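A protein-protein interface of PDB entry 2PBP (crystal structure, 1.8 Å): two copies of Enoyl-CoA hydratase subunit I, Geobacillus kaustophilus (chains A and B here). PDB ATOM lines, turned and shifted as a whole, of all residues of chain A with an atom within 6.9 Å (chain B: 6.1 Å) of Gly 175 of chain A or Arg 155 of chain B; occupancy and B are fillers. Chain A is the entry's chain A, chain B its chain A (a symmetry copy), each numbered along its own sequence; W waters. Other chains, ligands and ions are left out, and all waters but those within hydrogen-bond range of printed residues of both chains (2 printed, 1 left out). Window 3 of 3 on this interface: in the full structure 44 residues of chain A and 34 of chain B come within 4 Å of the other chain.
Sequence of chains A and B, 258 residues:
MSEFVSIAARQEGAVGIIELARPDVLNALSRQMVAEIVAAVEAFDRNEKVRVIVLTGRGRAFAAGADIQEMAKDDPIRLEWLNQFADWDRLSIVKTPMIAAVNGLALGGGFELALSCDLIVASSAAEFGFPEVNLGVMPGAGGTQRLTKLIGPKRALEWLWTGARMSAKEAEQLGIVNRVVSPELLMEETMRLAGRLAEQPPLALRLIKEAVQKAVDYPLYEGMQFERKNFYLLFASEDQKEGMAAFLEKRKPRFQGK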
ATOM      1  N   ASP A 118      -6.605  10.459  31.562  1.00  0.00           N
ATOM      2  CA  ASP A 118      -5.860  11.220  30.557  1.00  0.00           C
ATOM      3  C   ASP A 118      -4.361  11.292  30.802  1.00  0.00           C
ATOM      4  O   ASP A 118      -3.571  11.342  29.855  1.00  0.00           O
ATOM      5  CB  ASP A 118      -6.422  12.635  30.468  1.00  0.00           C
ATOM      6  CG  ASP A 118      -7.912  12.643  30.226  1.00  0.00           C
ATOM      7  OD1 ASP A 118      -8.349  12.003  29.246  1.00  0.00           O
ATOM      8  OD2 ASP A 118      -8.643  13.280  31.017  1.00  0.00           O
ATOM      9  N   LEU A 119      -3.982  11.329  32.073  1.00  0.00           N
ATOM     10  CA  LEU A 119      -2.581  11.385  32.468  1.00  0.00           C
ATOM     11  C   LEU A 119      -2.417  10.433  33.632  1.00  0.00           C
ATOM     12  O   LEU A 119      -3.355  10.221  34.406  1.00  0.00           O
ATOM     13  CB  LEU A 119      -2.192  12.790  32.937  1.00  0.00           C
ATOM     14  CG  LEU A 119      -2.364  13.982  31.996  1.00  0.00           C
ATOM     15  CD1 LEU A 119      -2.013  15.261  32.735  1.00  0.00           C
ATOM     16  CD2 LEU A 119      -1.481  13.809  30.771  1.00  0.00           C
ATOM     17  N   LEU A 150      -1.005   2.556  22.483  1.00  0.00           N
ATOM     18  CA  LEU A 150       0.087   3.277  23.123  1.00  0.00           C
ATOM     19  C   LEU A 150       1.492   2.766  22.820  1.00  0.00           C
ATOM     20  O   LEU A 150       2.404   3.563  22.609  1.00  0.00           O
ATOM     21  CB  LEU A 150      -0.108   3.298  24.642  1.00  0.00           C
ATOM     22  CG  LEU A 150      -1.217   4.199  25.189  1.00  0.00           C
ATOM     23  CD1 LEU A 150      -1.400   3.934  26.676  1.00  0.00           C
ATOM     24  CD2 LEU A 150      -0.854   5.660  24.946  1.00  0.00           C
ATOM     25  N   ILE A 151       1.676   1.447  22.796  1.00  0.00           N
ATOM     26  CA  ILE A 151       3.011   0.903  22.565  1.00  0.00           C
ATOM     27  C   ILE A 151       3.209  -0.008  21.353  1.00  0.00           C
ATOM     28  O   ILE A 151       4.294  -0.560  21.163  1.00  0.00           O
ATOM     29  CB  ILE A 151       3.511   0.181  23.852  1.00  0.00           C
ATOM     30  CG1 ILE A 151       2.647  -1.040  24.168  1.00  0.00           C
ATOM     31  CG2 ILE A 151       3.399   1.126  25.044  1.00  0.00           C
ATOM     32  CD1 ILE A 151       3.280  -2.047  25.130  1.00  0.00           C
ATOM     33  N   GLU A 170       9.408   1.509  33.266  1.00  0.00           N
ATOM     34  CA  GLU A 170       9.288   1.141  31.861  1.00  0.00           C
ATOM     35  C   GLU A 170       8.003   1.712  31.287  1.00  0.00           C
ATOM     36  O   GLU A 170       7.944   2.058  30.109  1.00  0.00           O
ATOM     37  CB  GLU A 170       9.303  -0.375  31.659  1.00  0.00           C
ATOM     38  CG  GLU A 170       9.672  -0.741  30.224  1.00  0.00           C
ATOM     39  CD  GLU A 170       9.620  -2.227  29.948  1.00  0.00           C
ATOM     40  OE1 GLU A 170       9.898  -3.016  30.872  1.00  0.00           O
ATOM     41  OE2 GLU A 170       9.316  -2.602  28.793  1.00  0.00           O
ATOM     42  N   ALA A 171       6.976   1.810  32.126  1.00  0.00           N
ATOM     43  CA  ALA A 171       5.697   2.361  31.696  1.00  0.00           C
ATOM     44  C   ALA A 171       5.906   3.812  31.273  1.00  0.00           C
ATOM     45  O   ALA A 171       5.297   4.285  30.314  1.00  0.00           O
ATOM     46  CB  ALA A 171       4.680   2.279  32.829  1.00  0.00           C
ATOM     47  N   GLU A 172       6.775   4.516  31.992  1.00  0.00           N
ATOM     48  CA  GLU A 172       7.064   5.908  31.670  1.00  0.00           C
ATOM     49  C   GLU A 172       7.878   5.995  30.386  1.00  0.00           C
ATOM     50  O   GLU A 172       7.628   6.854  29.545  1.00  0.00           O
ATOM     51  CB  GLU A 172       7.838   6.581  32.805  1.00  0.00           C
ATOM     52  CG  GLU A 172       8.268   8.001  32.461  1.00  0.00           C
ATOM     53  CD  GLU A 172       9.087   8.648  33.554  1.00  0.00           C
ATOM     54  OE1 GLU A 172      10.057   8.015  34.015  1.00  0.00           O
ATOM     55  OE2 GLU A 172       8.763   9.792  33.945  1.00  0.00           O
ATOM     56  N   GLN A 173       8.850   5.102  30.238  1.00  0.00           N
ATOM     57  CA  GLN A 173       9.692   5.089  29.045  1.00  0.00           C
ATOM     58  C   GLN A 173       8.857   4.788  27.801  1.00  0.00           C
ATOM     59  O   GLN A 173       9.159   5.272  26.708  1.00  0.00           O
ATOM     60  CB  GLN A 173      10.796   4.036  29.183  1.00  0.00           C
ATOM     61  CG  GLN A 173      11.710   4.201  30.395  1.00  0.00           C
ATOM     62  CD  GLN A 173      12.449   5.529  30.416  1.00  0.00           C
ATOM     63  OE1 GLN A 173      11.977   6.509  30.998  1.00  0.00           O
ATOM     64  NE2 GLN A 173      13.611   5.568  29.774  1.00  0.00           N
ATOM     65  N   LEU A 174       7.805   3.992  27.976  1.00  0.00           N
ATOM     66  CA  LEU A 174       6.925   3.622  26.872  1.00  0.00           C
ATOM     67  C   LEU A 174       5.887   4.694  26.563  1.00  0.00           C
ATOM     68  O   LEU A 174       5.181   4.611  25.558  1.00  0.00           O
ATOM     69  CB  LEU A 174       6.224   2.292  27.179  1.00  0.00           C
ATOM     70  CG  LEU A 174       7.109   1.042  27.210  1.00  0.00           C
ATOM     71  CD1 LEU A 174       6.306  -0.148  27.711  1.00  0.00           C
ATOM     72  CD2 LEU A 174       7.665   0.768  25.819  1.00  0.00           C
ATOM     73  N   GLY A 175       5.790   5.701  27.425  1.00  0.00           N
ATOM     74  CA  GLY A 175       4.834   6.767  27.191  1.00  0.00           C
ATOM     75  C   GLY A 175       3.454   6.502  27.762  1.00  0.00           C
ATOM     76  O   GLY A 175       2.483   7.168  27.399  1.00  0.00           O
ATOM     77  N   ILE A 176       3.363   5.513  28.646  1.00  0.00           N
ATOM     78  CA  ILE A 176       2.096   5.177  29.282  1.00  0.00           C
ATOM     79  C   ILE A 176       1.929   6.047  30.529  1.00  0.00           C
ATOM     80  O   ILE A 176       0.847   6.582  30.786  1.00  0.00           O
ATOM     81  CB  ILE A 176       2.060   3.693  29.695  1.00  0.00           C
ATOM     82  CG1 ILE A 176       2.205   2.810  28.451  1.00  0.00           C
ATOM     83  CG2 ILE A 176       0.759   3.392  30.433  1.00  0.00           C
ATOM     84  CD1 ILE A 176       2.522   1.344  28.738  1.00  0.00           C
ATOM     85  N   VAL A 177       3.009   6.176  31.294  1.00  0.00           N
ATOM     86  CA  VAL A 177       3.018   6.983  32.512  1.00  0.00           C
ATOM     87  C   VAL A 177       3.725   8.310  32.237  1.00  0.00           C
ATOM     88  O   VAL A 177       4.768   8.345  31.581  1.00  0.00           O
ATOM     89  CB  VAL A 177       3.734   6.242  33.668  1.00  0.00           C
ATOM     90  CG1 VAL A 177       4.061   7.211  34.802  1.00  0.00           C
ATOM     91  CG2 VAL A 177       2.838   5.119  34.193  1.00  0.00           C
ATOM     92  N   ASN A 178       3.152   9.398  32.739  1.00  0.00           N
ATOM     93  CA  ASN A 178       3.717  10.727  32.518  1.00  0.00           C
ATOM     94  C   ASN A 178       4.914  11.046  33.412  1.00  0.00           C
ATOM     95  O   ASN A 178       5.861  11.709  32.980  1.00  0.00           O
ATOM     96  CB  ASN A 178       2.621  11.780  32.685  1.00  0.00           C
ATOM     97  CG  ASN A 178       1.577  11.713  31.572  1.00  0.00           C
ATOM     98  OD1 ASN A 178       1.791  12.221  30.470  1.00  0.00           O
ATOM     99  ND2 ASN A 178       0.453  11.070  31.854  1.00  0.00           N
ATOM    100  N   LEU B 147       0.391  15.575  16.681  1.00  0.00           N
ATOM    101  CA  LEU B 147       1.173  15.283  17.881  1.00  0.00           C
ATOM    102  C   LEU B 147       0.696  13.990  18.541  1.00  0.00           C
ATOM    103  O   LEU B 147       1.504  13.150  18.936  1.00  0.00           O
ATOM    104  CB  LEU B 147       1.088  16.435  18.894  1.00  0.00           C
ATOM    105  CG  LEU B 147       2.074  16.321  20.067  1.00  0.00           C
ATOM    106  CD1 LEU B 147       3.494  16.511  19.545  1.00  0.00           C
ATOM    107  CD2 LEU B 147       1.774  17.373  21.131  1.00  0.00           C
ATOM    108  N   LEU B 150       1.792  10.896  16.740  1.00  0.00           N
ATOM    109  CA  LEU B 150       3.219  10.646  16.890  1.00  0.00           C
ATOM    110  C   LEU B 150       3.667  10.151  18.262  1.00  0.00           C
ATOM    111  O   LEU B 150       4.508   9.257  18.348  1.00  0.00           O
ATOM    112  CB  LEU B 150       4.019  11.905  16.541  1.00  0.00           C
ATOM    113  CG  LEU B 150       4.095  12.292  15.063  1.00  0.00           C
ATOM    114  CD1 LEU B 150       4.743  13.663  14.929  1.00  0.00           C
ATOM    115  CD2 LEU B 150       4.900  11.243  14.302  1.00  0.00           C
ATOM    116  N   ILE B 151       3.117  10.719  19.333  1.00  0.00           N
ATOM    117  CA  ILE B 151       3.549  10.322  20.670  1.00  0.00           C
ATOM    118  C   ILE B 151       2.495   9.747  21.617  1.00  0.00           C
ATOM    119  O   ILE B 151       2.790   9.476  22.783  1.00  0.00           O
ATOM    120  CB  ILE B 151       4.280  11.513  21.359  1.00  0.00           C
ATOM    121  CG1 ILE B 151       3.324  12.682  21.595  1.00  0.00           C
ATOM    122  CG2 ILE B 151       5.392  12.025  20.450  1.00  0.00           C
ATOM    123  CD1 ILE B 151       3.802  13.709  22.622  1.00  0.00           C
ATOM    124  N   GLY B 152       1.274   9.562  21.124  1.00  0.00           N
ATOM    125  CA  GLY B 152       0.223   9.007  21.961  1.00  0.00           C
ATOM    126  C   GLY B 152      -0.542  10.060  22.743  1.00  0.00           C
ATOM    127  O   GLY B 152      -0.014  11.140  22.996  1.00  0.00           O
ATOM    128  N   PRO B 153      -1.785   9.769  23.160  1.00  0.00           N
ATOM    129  CA  PRO B 153      -2.605  10.724  23.915  1.00  0.00           C
ATOM    130  C   PRO B 153      -2.111  11.097  25.313  1.00  0.00           C
ATOM    131  O   PRO B 153      -2.310  12.230  25.760  1.00  0.00           O
ATOM    132  CB  PRO B 153      -3.970  10.045  23.951  1.00  0.00           C
ATOM    133  CG  PRO B 153      -3.607   8.598  24.017  1.00  0.00           C
ATOM    134  CD  PRO B 153      -2.500   8.493  22.983  1.00  0.00           C
ATOM    135  N   LYS B 154      -1.481  10.153  26.007  1.00  0.00           N
ATOM    136  CA  LYS B 154      -0.980  10.410  27.359  1.00  0.00           C
ATOM    137  C   LYS B 154       0.068  11.527  27.356  1.00  0.00           C
ATOM    138  O   LYS B 154      -0.020  12.491  28.123  1.00  0.00           O
ATOM    139  CB  LYS B 154      -0.378   9.129  27.957  1.00  0.00           C
ATOM    140  CG  LYS B 154      -1.391   8.014  28.233  1.00  0.00           C
ATOM    141  CD  LYS B 154      -2.196   8.285  29.502  1.00  0.00           C
ATOM    142  CE  LYS B 154      -3.223   7.191  29.775  1.00  0.00           C
ATOM    143  NZ  LYS B 154      -4.353   7.208  28.794  1.00  0.00           N
ATOM    144  N   ARG B 155       1.062  11.405  26.484  1.00  0.00           N
ATOM    145  CA  ARG B 155       2.099  12.419  26.413  1.00  0.00           C
ATOM    146  C   ARG B 155       1.610  13.683  25.705  1.00  0.00           C
ATOM    147  O   ARG B 155       1.945  14.796  26.105  1.00  0.00           O
ATOM    148  CB  ARG B 155       3.344  11.843  25.726  1.00  0.00           C
ATOM    149  CG  ARG B 155       4.053  10.798  26.584  1.00  0.00           C
ATOM    150  CD  ARG B 155       5.292  10.220  25.923  1.00  0.00           C
ATOM    151  NE  ARG B 155       4.953   9.464  24.725  1.00  0.00           N
ATOM    152  CZ  ARG B 155       5.714   8.508  24.202  1.00  0.00           C
ATOM    153  NH1 ARG B 155       6.864   8.187  24.777  1.00  0.00           N
ATOM    154  NH2 ARG B 155       5.320   7.873  23.106  1.00  0.00           N
ATOM    155  N   ALA B 156       0.786  13.512  24.677  1.00  0.00           N
ATOM    156  CA  ALA B 156       0.272  14.652  23.925  1.00  0.00           C
ATOM    157  C   ALA B 156      -0.515  15.624  24.793  1.00  0.00           C
ATOM    158  O   ALA B 156      -0.317  16.837  24.705  1.00  0.00           O
ATOM    159  CB  ALA B 156      -0.600  14.170  22.776  1.00  0.00           C
ATOM    160  N   LEU B 157      -1.409  15.098  25.625  1.00  0.00           N
ATOM    161  CA  LEU B 157      -2.224  15.958  26.482  1.00  0.00           C
ATOM    162  C   LEU B 157      -1.381  16.757  27.466  1.00  0.00           C
ATOM    163  O   LEU B 157      -1.725  17.886  27.814  1.00  0.00           O
ATOM    164  CB  LEU B 157      -3.279  15.131  27.222  1.00  0.00           C
ATOM    165  CG  LEU B 157      -4.443  14.683  26.327  1.00  0.00           C
ATOM    166  CD1 LEU B 157      -5.359  13.740  27.090  1.00  0.00           C
ATOM    167  CD2 LEU B 157      -5.211  15.916  25.841  1.00  0.00           C
ATOM    168  N   GLU B 158      -0.270  16.177  27.902  1.00  0.00           N
ATOM    169  CA  GLU B 158       0.621  16.865  28.826  1.00  0.00           C
ATOM    170  C   GLU B 158       1.099  18.158  28.155  1.00  0.00           C
ATOM    171  O   GLU B 158       0.988  19.249  28.719  1.00  0.00           O
ATOM    172  CB  GLU B 158       1.822  15.970  29.157  1.00  0.00           C
ATOM    173  CG  GLU B 158       2.684  16.463  30.308  1.00  0.00           C
ATOM    174  CD  GLU B 158       3.931  15.616  30.507  1.00  0.00           C
ATOM    175  OE1 GLU B 158       3.816  14.374  30.517  1.00  0.00           O
ATOM    176  OE2 GLU B 158       5.028  16.193  30.656  1.00  0.00           O
ATOM    177  N   TRP B 159       1.611  18.037  26.935  1.00  0.00           N
ATOM    178  CA  TRP B 159       2.108  19.201  26.215  1.00  0.00           C
ATOM    179  C   TRP B 159       1.022  20.173  25.769  1.00  0.00           C
ATOM    180  O   TRP B 159       1.197  21.388  25.858  1.00  0.00           O
ATOM    181  CB  TRP B 159       2.926  18.757  24.999  1.00  0.00           C
ATOM    182  CG  TRP B 159       4.129  17.956  25.380  1.00  0.00           C
ATOM    183  CD1 TRP B 159       4.260  16.598  25.343  1.00  0.00           C
ATOM    184  CD2 TRP B 159       5.357  18.464  25.908  1.00  0.00           C
ATOM    185  NE1 TRP B 159       5.496  16.227  25.816  1.00  0.00           N
ATOM    186  CE2 TRP B 159       6.190  17.354  26.170  1.00  0.00           C
ATOM    187  CE3 TRP B 159       5.836  19.749  26.188  1.00  0.00           C
ATOM    188  CZ2 TRP B 159       7.479  17.490  26.699  1.00  0.00           C
ATOM    189  CZ3 TRP B 159       7.120  19.888  26.715  1.00  0.00           C
ATOM    190  CH2 TRP B 159       7.924  18.761  26.965  1.00  0.00           C
ATOM    191  N   LEU B 160      -0.095  19.637  25.287  1.00  0.00           N
ATOM    192  CA  LEU B 160      -1.194  20.468  24.808  1.00  0.00           C
ATOM    193  C   LEU B 160      -1.913  21.224  25.925  1.00  0.00           C
ATOM    194  O   LEU B 160      -2.300  22.377  25.745  1.00  0.00           O
ATOM    195  CB  LEU B 160      -2.192  19.604  24.029  1.00  0.00           C
ATOM    196  CG  LEU B 160      -1.638  18.996  22.734  1.00  0.00           C
ATOM    197  CD1 LEU B 160      -2.562  17.897  22.234  1.00  0.00           C
ATOM    198  CD2 LEU B 160      -1.485  20.096  21.683  1.00  0.00           C
ATOM    199  N   LEU B 174      11.339  11.312  21.045  1.00  0.00           N
ATOM    200  CA  LEU B 174       9.940  10.945  20.850  1.00  0.00           C
ATOM    201  C   LEU B 174       9.631  10.547  19.412  1.00  0.00           C
ATOM    202  O   LEU B 174       8.542  10.052  19.119  1.00  0.00           O
ATOM    203  CB  LEU B 174       9.026  12.101  21.277  1.00  0.00           C
ATOM    204  CG  LEU B 174       8.984  12.424  22.774  1.00  0.00           C
ATOM    205  CD1 LEU B 174       8.192  13.703  23.005  1.00  0.00           C
ATOM    206  CD2 LEU B 174       8.362  11.261  23.536  1.00  0.00           C
HETATM  207  O   HOH W   1       8.087   9.071  27.303  1.00  0.00           O
HETATM  208  O   HOH W   2      -4.485   9.750  27.571  1.00  0.00           O
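The side-chain amide oxygen of Asn 178 of chain A lies close to the backbone carbonyl oxygen of Lys 154 of chain B (3.0 Å). The side-chain carboxylate (OE1) of Glu 158 of chain B sits close to the side-chain amide oxygen (OD1) of Asn 178 of chain A (3.0 Å).
The backbone carbonyl oxygen of Ala 171 of chain A is in hydrogen-bond range of the backbone NH of Ile 176 of chain A, at 2.8 Å. NE of Arg 155 of chain B lies within hydrogen-bond range of O of Ile 151 of chain B (2.9 Å).
Lys 154 of chain B touches Asp 118 of chain A. Asp 118 of chain A touches Leu 157 of chain B. CD2 of Leu 119 of chain A touches O of Lys 154 of chain B, 3.3 Å away. Leu 119 of chain A touches Glu 158 of chain B (CD2 to N, 3.9 Å). Leu 150 of chain A touches Pro 153 of chain B (CD2 to CD, 3.8 Å). Lys 154 of chain B touches Gly 175 of chain A. Gly 175 of chain A touches Arg 155 of chain B. Ile 176 of chain A touches Lys 154 of chain B (O to CG, 3.7 Å).
Of chain B, only Lys 154 (3.5 Å) and Arg 155 (3.5 Å) come within 4 Å of Gly 175 of chain A. Printed residues of chain B within 4 Å of Leu 150 of chain A: Pro 153 (3.8 Å). Of the printed residues of chain B, Ile 176 of chain A touches Lys 154. The nearest residue of chain B that does not touch Gly 175 of chain A is Ile 151 of chain B (5.2 Å). The nearest printed residue of chain A that does not touch Glu 158 of chain B is Asp 118 of chain A (6.2 Å).
Along chain B the printed residues that touch a printed residue of chain A span positions 153 to 158. Hydrophobic or aromatic side chains of chain A that line the printed part of chain B: Leu 119 and Leu 150. Among the printed residues, 10 pairs touch across the chains. Among the printed residues, no Asp or Glu carboxylate lies within 4 Å of a Lys or Arg side-chain nitrogen of the other chain.
Positions printed for both chains: 150, 151 and 174. Of the 10 pairs that touch across the chains among the printed residues, none has its exchanged pair printed and touching as well.
Water W2 bridges NZ of Lys 154 of chain B and O of Asp 118 of chain A. Water W1 bridges the guanidinium group (NH1) of Arg 155 of chain B (2.9 Å) and the backbone carbonyl oxygen (O) of Glu 172 of chain A (3.2 Å).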
